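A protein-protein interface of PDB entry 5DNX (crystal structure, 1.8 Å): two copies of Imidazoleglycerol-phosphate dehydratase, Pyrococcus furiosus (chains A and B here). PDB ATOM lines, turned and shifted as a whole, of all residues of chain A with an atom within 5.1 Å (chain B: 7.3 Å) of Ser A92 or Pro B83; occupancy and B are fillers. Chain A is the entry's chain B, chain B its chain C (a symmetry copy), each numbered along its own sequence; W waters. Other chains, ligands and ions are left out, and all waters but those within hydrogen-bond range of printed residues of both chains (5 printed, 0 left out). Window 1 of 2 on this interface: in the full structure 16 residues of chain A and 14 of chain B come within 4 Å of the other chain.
The backbone carbonyl oxygen (O) of Ala B87 is in hydrogen-bond range of a ring nitrogen (NE2) of His A135, at 3.5 Å.
The backbone carbonyl oxygen of Asp B85 is in hydrogen-bond range of a ring nitrogen (NE2) of His A135 (2.8 Å).
ND2 of Asn A79 is in hydrogen-bond range of O of Ile B81 (2.9 Å).
Of the printed residues of chain B, Ser A92 touches Pro B83 and Leu B88.
Printed residues of chain B within 4 Å of Phe A77: Met B82 (3.5 Å).
Printed residues of chain A within 4 Å of Leu B88: Leu A90 (3.9 Å), Ser A92 (3.5 Å) and His A135 (3.997 Å).
Of the printed residues of chain A, Asp B85 touches Thr A133 (3.6 Å) and His A135 (2.8 Å).
The nearest printed residue of chain B that does not touch Ser A92 is Ile B81 (4.02 Å).
The nearest printed residue of chain A that does not touch Pro B83 is Val A93 (4.001 Å).
The nearest printed residue of chain B that does not touch Asp A94 is Met B84 (5.0 Å).
A ring nitrogen (ND1) of His B146 is in hydrogen-bond range of the side-chain carboxylate of Asp B86, 2.7 Å away.
O of Ser A92 is in hydrogen-bond range of N of His A135 (2.9 Å).
N of Thr A133 lies within hydrogen-bond range of O of Asp A94, at 2.8 Å.
OD1 of Asn A79 lies within hydrogen-bond range of OG of Ser A92.
The backbone NH of Met B82 lies within hydrogen-bond range of the backbone carbonyl oxygen of Val B89.
Among the printed residues, merely in contact across the chains: Ser A92 with Pro B83 (3.2 Å), His A135 with Asp B86 (3.4 Å), Phe A77 with Met B82 (3.5 Å), Ser A92 with Leu B88 (3.5 Å), Thr A133 with Asp B85 (3.6 Å), Asp A94 with Pro B83 (3.7 Å), Leu A90 with Ile B81 (3.8 Å), His A135 with Pro B83 (3.9 Å), Leu A90 with Leu B88 (3.9 Å) and His A135 with Leu B88 (3.997 Å).
Hydrophobic or aromatic side chains of chain A within 4 Å of the printed part of chain B: Phe A77, Leu A90 and His A135.
Of the 12 printed residues of chain B, 7 touch a printed residue of chain A.
Hydrophobic or aromatic side chains of chain B within 4 Å of the printed part of chain A: Ile B81, Met B82, Pro B83 and Leu B88.
Among the printed residues, 13 pairs touch across the chains.
Water W5 bridges OG1 of Thr A133 (2.5 Å) and OD1 of Asp B85 (2.6 Å).
Water W4 lies within hydrogen-bond range of the side-chain carboxylate of Asp A94 (2.7 Å), the side-chain hydroxyl of Thr A133 (2.9 Å) and the backbone NH of Asp B85 (3.1 Å).
Water W1 lies within hydrogen-bond range of OD2 of Asp A94 (2.8 Å), NZ of Lys B153 (2.8 Å) and O of Pro B83 (2.8 Å).
Water W2 bridges the backbone carbonyl oxygen (O) of Ile B81 (2.9 Å) and the side-chain amide nitrogen (ND2) of Asn A79 (3.5 Å).
Water W3 bridges N of Ile B81 (3.0 Å) and ND2 of Asn A79 (3.1 Å).
No position is printed for both chains.
Of the 13 pairs that touch across the chains among the printed residues, none has its exchanged pair printed and touching as well.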
ATOM      1  N   PHE A  77      21.027 -24.140  21.130  1.00  0.00           N
ATOM      2  CA  PHE A  77      20.299 -23.704  19.944  1.00  0.00           C
ATOM      3  C   PHE A  77      20.323 -22.213  19.788  1.00  0.00           C
ATOM      4  O   PHE A  77      20.156 -21.460  20.756  1.00  0.00           O
ATOM      5  CB  PHE A  77      18.846 -24.181  20.019  1.00  0.00           C
ATOM      6  CG  PHE A  77      18.704 -25.675  19.909  1.00  0.00           C
ATOM      7  CD1 PHE A  77      18.748 -26.298  18.686  1.00  0.00           C
ATOM      8  CD2 PHE A  77      18.521 -26.469  21.052  1.00  0.00           C
ATOM      9  CE1 PHE A  77      18.609 -27.669  18.580  1.00  0.00           C
ATOM     10  CE2 PHE A  77      18.390 -27.858  20.957  1.00  0.00           C
ATOM     11  CZ  PHE A  77      18.413 -28.465  19.719  1.00  0.00           C
ATOM     12  N   GLY A  78      20.479 -21.753  18.555  1.00  0.00           N
ATOM     13  CA  GLY A  78      20.263 -20.338  18.268  1.00  0.00           C
ATOM     14  C   GLY A  78      19.916 -20.115  16.808  1.00  0.00           C
ATOM     15  O   GLY A  78      20.442 -20.806  15.953  1.00  0.00           O
ATOM     16  N   ASN A  79      19.055 -19.136  16.555  1.00  0.00           N
ATOM     17  CA  ASN A  79      18.664 -18.769  15.188  1.00  0.00           C
ATOM     18  C   ASN A  79      18.782 -17.284  14.952  1.00  0.00           C
ATOM     19  O   ASN A  79      18.772 -16.493  15.878  1.00  0.00           O
ATOM     20  CB  ASN A  79      17.228 -19.172  14.882  1.00  0.00           C
ATOM     21  CG  ASN A  79      16.977 -20.630  15.040  1.00  0.00           C
ATOM     22  OD1 ASN A  79      17.661 -21.467  14.455  1.00  0.00           O
ATOM     23  ND2 ASN A  79      15.976 -20.956  15.837  1.00  0.00           N
ATOM     24  N   ALA A  80      18.902 -16.905  13.687  1.00  0.00           N
ATOM     25  CA  ALA A  80      18.735 -15.510  13.291  1.00  0.00           C
ATOM     26  C   ALA A  80      18.148 -15.465  11.897  1.00  0.00           C
ATOM     27  O   ALA A  80      18.447 -16.318  11.069  1.00  0.00           O
ATOM     28  CB  ALA A  80      20.071 -14.806  13.313  1.00  0.00           C
ATOM     29  N   LEU A  90      18.228 -16.946   6.596  1.00  0.00           N
ATOM     30  CA  LEU A  90      17.977 -17.667   7.836  1.00  0.00           C
ATOM     31  C   LEU A  90      19.251 -18.413   8.208  1.00  0.00           C
ATOM     32  O   LEU A  90      19.801 -19.129   7.387  1.00  0.00           O
ATOM     33  CB  LEU A  90      16.819 -18.648   7.674  1.00  0.00           C
ATOM     34  CG  LEU A  90      16.628 -19.735   8.762  1.00  0.00           C
ATOM     35  CD1 LEU A  90      16.382 -19.102  10.128  1.00  0.00           C
ATOM     36  CD2 LEU A  90      15.514 -20.683   8.349  1.00  0.00           C
ATOM     37  N   VAL A  91      19.680 -18.256   9.454  1.00  0.00           N
ATOM     38  CA  VAL A  91      20.816 -18.986  10.015  1.00  0.00           C
ATOM     39  C   VAL A  91      20.315 -19.730  11.232  1.00  0.00           C
ATOM     40  O   VAL A  91      19.711 -19.144  12.128  1.00  0.00           O
ATOM     41  CB  VAL A  91      21.968 -18.034  10.405  1.00  0.00           C
ATOM     42  CG1 VAL A  91      23.131 -18.812  11.028  1.00  0.00           C
ATOM     43  CG2 VAL A  91      22.431 -17.275   9.168  1.00  0.00           C
ATOM     44  N   SER A  92      20.533 -21.033  11.244  1.00  0.00           N
ATOM     45  CA  SER A  92      20.049 -21.876  12.319  1.00  0.00           C
ATOM     46  C   SER A  92      21.174 -22.774  12.795  1.00  0.00           C
ATOM     47  O   SER A  92      21.765 -23.505  11.999  1.00  0.00           O
ATOM     48  CB  SER A  92      18.831 -22.683  11.855  1.00  0.00           C
ATOM     49  OG  SER A  92      18.302 -23.502  12.897  1.00  0.00           O
ATOM     50  N   VAL A  93      21.471 -22.702  14.093  1.00  0.00           N
ATOM     51  CA  VAL A  93      22.599 -23.427  14.683  1.00  0.00           C
ATOM     52  C   VAL A  93      22.119 -24.343  15.798  1.00  0.00           C
ATOM     53  O   VAL A  93      21.270 -23.960  16.616  1.00  0.00           O
ATOM     54  CB  VAL A  93      23.636 -22.428  15.253  1.00  0.00           C
ATOM     55  CG1 VAL A  93      24.724 -23.118  16.055  1.00  0.00           C
ATOM     56  CG2 VAL A  93      24.241 -21.627  14.097  1.00  0.00           C
ATOM     57  N   ASP A  94      22.716 -25.535  15.852  1.00  0.00           N
ATOM     58  CA  ASP A  94      22.574 -26.460  16.976  1.00  0.00           C
ATOM     59  C   ASP A  94      23.994 -26.931  17.317  1.00  0.00           C
ATOM     60  O   ASP A  94      24.607 -27.614  16.511  1.00  0.00           O
ATOM     61  CB  ASP A  94      21.669 -27.630  16.560  1.00  0.00           C
ATOM     62  CG  ASP A  94      21.698 -28.782  17.524  1.00  0.00           C
ATOM     63  OD1 ASP A  94      22.393 -28.657  18.564  1.00  0.00           O
ATOM     64  OD2 ASP A  94      21.035 -29.830  17.246  1.00  0.00           O
ATOM     65  N   THR A 133      25.858 -28.278  14.079  1.00  0.00           N
ATOM     66  CA  THR A 133      24.968 -28.336  12.928  1.00  0.00           C
ATOM     67  C   THR A 133      24.666 -26.904  12.520  1.00  0.00           C
ATOM     68  O   THR A 133      24.205 -26.106  13.349  1.00  0.00           O
ATOM     69  CB  THR A 133      23.633 -28.987  13.353  1.00  0.00           C
ATOM     70  OG1 THR A 133      23.857 -30.282  13.953  1.00  0.00           O
ATOM     71  CG2 THR A 133      22.671 -29.103  12.188  1.00  0.00           C
ATOM     72  N   ILE A 134      24.916 -26.540  11.256  1.00  0.00           N
ATOM     73  CA  ILE A 134      24.694 -25.150  10.832  1.00  0.00           C
ATOM     74  C   ILE A 134      23.940 -25.148   9.508  1.00  0.00           C
ATOM     75  O   ILE A 134      24.412 -25.724   8.541  1.00  0.00           O
ATOM     76  CB  ILE A 134      26.012 -24.357  10.662  1.00  0.00           C
ATOM     77  CG1 ILE A 134      26.870 -24.432  11.941  1.00  0.00           C
ATOM     78  CG2 ILE A 134      25.709 -22.918  10.253  1.00  0.00           C
ATOM     79  CD1 ILE A 134      28.175 -23.648  11.846  1.00  0.00           C
ATOM     80  N   HIS A 135      22.774 -24.497   9.494  1.00  0.00           N
ATOM     81  CA  HIS A 135      22.010 -24.250   8.285  1.00  0.00           C
ATOM     82  C   HIS A 135      22.070 -22.773   7.944  1.00  0.00           C
ATOM     83  O   HIS A 135      21.864 -21.926   8.804  1.00  0.00           O
ATOM     84  CB  HIS A 135      20.546 -24.605   8.471  1.00  0.00           C
ATOM     85  CG  HIS A 135      20.279 -26.060   8.450  1.00  0.00           C
ATOM     86  ND1 HIS A 135      19.915 -26.721   7.295  1.00  0.00           N
ATOM     87  CD2 HIS A 135      20.323 -26.993   9.425  1.00  0.00           C
ATOM     88  CE1 HIS A 135      19.762 -28.002   7.561  1.00  0.00           C
ATOM     89  NE2 HIS A 135      19.991 -28.193   8.845  1.00  0.00           N
ATOM     90  N   ILE B  81      12.396 -22.400  15.229  1.00  0.00           N
ATOM     91  CA  ILE B  81      13.003 -23.005  14.068  1.00  0.00           C
ATOM     92  C   ILE B  81      14.033 -23.974  14.616  1.00  0.00           C
ATOM     93  O   ILE B  81      14.965 -23.581  15.323  1.00  0.00           O
ATOM     94  CB  ILE B  81      13.632 -21.968  13.154  1.00  0.00           C
ATOM     95  CG1 ILE B  81      12.524 -21.131  12.503  1.00  0.00           C
ATOM     96  CG2 ILE B  81      14.462 -22.666  12.058  1.00  0.00           C
ATOM     97  CD1 ILE B  81      13.048 -19.906  11.782  1.00  0.00           C
ATOM     98  N   MET B  82      13.812 -25.244  14.318  1.00  0.00           N
ATOM     99  CA  MET B  82      14.568 -26.331  14.894  1.00  0.00           C
ATOM    100  C   MET B  82      15.384 -27.044  13.821  1.00  0.00           C
ATOM    101  O   MET B  82      14.795 -27.668  12.923  1.00  0.00           O
ATOM    102  CB  MET B  82      13.588 -27.306  15.547  1.00  0.00           C
ATOM    103  CG  MET B  82      14.259 -28.309  16.447  1.00  0.00           C
ATOM    104  SD  MET B  82      15.267 -27.501  17.710  1.00  0.00           S
ATOM    105  CE  MET B  82      14.259 -26.066  18.147  1.00  0.00           C
ATOM    106  N   PRO B  83      16.730 -26.959  13.902  1.00  0.00           N
ATOM    107  CA  PRO B  83      17.575 -27.772  13.066  1.00  0.00           C
ATOM    108  C   PRO B  83      17.776 -29.124  13.731  1.00  0.00           C
ATOM    109  O   PRO B  83      17.839 -29.213  14.959  1.00  0.00           O
ATOM    110  CB  PRO B  83      18.873 -26.983  13.000  1.00  0.00           C
ATOM    111  CG  PRO B  83      18.957 -26.313  14.339  1.00  0.00           C
ATOM    112  CD  PRO B  83      17.535 -26.041  14.748  1.00  0.00           C
ATOM    113  N   MET B  84      17.827 -30.175  12.939  1.00  0.00           N
ATOM    114  CA  MET B  84      18.305 -31.458  13.444  1.00  0.00           C
ATOM    115  C   MET B  84      19.004 -32.169  12.332  1.00  0.00           C
ATOM    116  O   MET B  84      18.372 -32.742  11.469  1.00  0.00           O
ATOM    117  CB  MET B  84      17.193 -32.305  14.029  1.00  0.00           C
ATOM    118  CG  MET B  84      17.790 -33.530  14.711  1.00  0.00           C
ATOM    119  SD  MET B  84      16.574 -34.526  15.555  1.00  0.00           S
ATOM    120  CE  MET B  84      17.654 -35.766  16.201  1.00  0.00           C
ATOM    121  N   ASP B  85      20.334 -32.130  12.363  1.00  0.00           N
ATOM    122  CA  ASP B  85      21.138 -32.555  11.220  1.00  0.00           C
ATOM    123  C   ASP B  85      20.563 -31.953   9.922  1.00  0.00           C
ATOM    124  O   ASP B  85      20.427 -30.733   9.837  1.00  0.00           O
ATOM    125  CB  ASP B  85      21.268 -34.094  11.201  1.00  0.00           C
ATOM    126  CG  ASP B  85      22.092 -34.648  12.368  1.00  0.00           C
ATOM    127  OD1 ASP B  85      22.462 -33.892  13.321  1.00  0.00           O
ATOM    128  OD2 ASP B  85      22.396 -35.872  12.306  1.00  0.00           O
ATOM    129  N   ASP B  86      20.195 -32.785   8.946  1.00  0.00           N
ATOM    130  CA  ASP B  86      19.608 -32.320   7.679  1.00  0.00           C
ATOM    131  C   ASP B  86      18.277 -31.592   7.807  1.00  0.00           C
ATOM    132  O   ASP B  86      17.952 -30.777   6.944  1.00  0.00           O
ATOM    133  CB  ASP B  86      19.393 -33.512   6.710  1.00  0.00           C
ATOM    134  CG  ASP B  86      18.557 -34.633   7.314  1.00  0.00           C
ATOM    135  OD1 ASP B  86      19.056 -35.328   8.235  1.00  0.00           O
ATOM    136  OD2 ASP B  86      17.394 -34.817   6.906  1.00  0.00           O
ATOM    137  N   ALA B  87      17.511 -31.869   8.868  1.00  0.00           N
ATOM    138  CA  ALA B  87      16.188 -31.260   9.029  1.00  0.00           C
ATOM    139  C   ALA B  87      16.269 -29.836   9.503  1.00  0.00           C
ATOM    140  O   ALA B  87      17.103 -29.481  10.338  1.00  0.00           O
ATOM    141  CB  ALA B  87      15.296 -32.056   9.984  1.00  0.00           C
ATOM    142  N   LEU B  88      15.357 -29.019   8.986  1.00  0.00           N
ATOM    143  CA  LEU B  88      15.175 -27.673   9.448  1.00  0.00           C
ATOM    144  C   LEU B  88      13.677 -27.420   9.402  1.00  0.00           C
ATOM    145  O   LEU B  88      13.090 -27.418   8.336  1.00  0.00           O
ATOM    146  CB  LEU B  88      15.914 -26.711   8.534  1.00  0.00           C
ATOM    147  CG  LEU B  88      15.920 -25.254   8.972  1.00  0.00           C
ATOM    148  CD1 LEU B  88      16.595 -25.111  10.321  1.00  0.00           C
ATOM    149  CD2 LEU B  88      16.594 -24.378   7.921  1.00  0.00           C
ATOM    150  N   VAL B  89      13.062 -27.256  10.569  1.00  0.00           N
ATOM    151  CA  VAL B  89      11.593 -27.212  10.676  1.00  0.00           C
ATOM    152  C   VAL B  89      11.145 -25.988  11.445  1.00  0.00           C
ATOM    153  O   VAL B  89      11.599 -25.734  12.566  1.00  0.00           O
ATOM    154  CB  VAL B  89      11.011 -28.489  11.348  1.00  0.00           C
ATOM    155  CG1 VAL B  89       9.489 -28.399  11.448  1.00  0.00           C
ATOM    156  CG2 VAL B  89      11.424 -29.767  10.603  1.00  0.00           C
ATOM    157  N   HIS B 146      14.670 -37.238  11.924  1.00  0.00           N
ATOM    158  CA  HIS B 146      15.139 -35.859  12.187  1.00  0.00           C
ATOM    159  C   HIS B 146      14.025 -34.838  11.966  1.00  0.00           C
ATOM    160  O   HIS B 146      13.898 -33.883  12.719  1.00  0.00           O
ATOM    161  CB  HIS B 146      16.343 -35.514  11.303  1.00  0.00           C
ATOM    162  CG  HIS B 146      17.527 -36.400  11.529  1.00  0.00           C
ATOM    163  ND1 HIS B 146      18.518 -36.559  10.590  1.00  0.00           N
ATOM    164  CD2 HIS B 146      17.891 -37.148  12.591  1.00  0.00           C
ATOM    165  CE1 HIS B 146      19.448 -37.370  11.065  1.00  0.00           C
ATOM    166  NE2 HIS B 146      19.087 -37.742  12.277  1.00  0.00           N
ATOM    167  N   ALA B 150      12.453 -32.934  15.055  1.00  0.00           N
ATOM    168  CA  ALA B 150      12.576 -31.468  15.011  1.00  0.00           C
ATOM    169  C   ALA B 150      11.225 -30.777  15.234  1.00  0.00           C
ATOM    170  O   ALA B 150      11.165 -29.756  15.910  1.00  0.00           O
ATOM    171  CB  ALA B 150      13.188 -30.995  13.692  1.00  0.00           C
ATOM    172  N   LYS B 153      10.483 -31.132  19.063  1.00  0.00           N
ATOM    173  CA  LYS B 153      11.362 -30.179  19.744  1.00  0.00           C
ATOM    174  C   LYS B 153      10.853 -28.758  19.549  1.00  0.00           C
ATOM    175  O   LYS B 153      10.799 -27.942  20.493  1.00  0.00           O
ATOM    176  CB  LYS B 153      12.794 -30.267  19.215  1.00  0.00           C
ATOM    177  CG  LYS B 153      13.575 -31.505  19.609  1.00  0.00           C
ATOM    178  CD  LYS B 153      14.913 -31.565  18.852  1.00  0.00           C
ATOM    179  CE  LYS B 153      15.941 -32.477  19.515  1.00  0.00           C
ATOM    180  NZ  LYS B 153      17.102 -32.749  18.598  1.00  0.00           N
HETATM  181  O   HOH W   1      18.481 -30.881  17.093  1.00  0.00           O
HETATM  182  O   HOH W   2      16.245 -23.727  17.885  1.00  0.00           O
HETATM  183  O   HOH W   3      13.790 -21.939  17.796  1.00  0.00           O
HETATM  184  O   HOH W   4      21.457 -31.365  15.101  1.00  0.00           O
HETATM  185  O   HOH W   5      24.338 -32.243  12.538  1.00  0.00           O
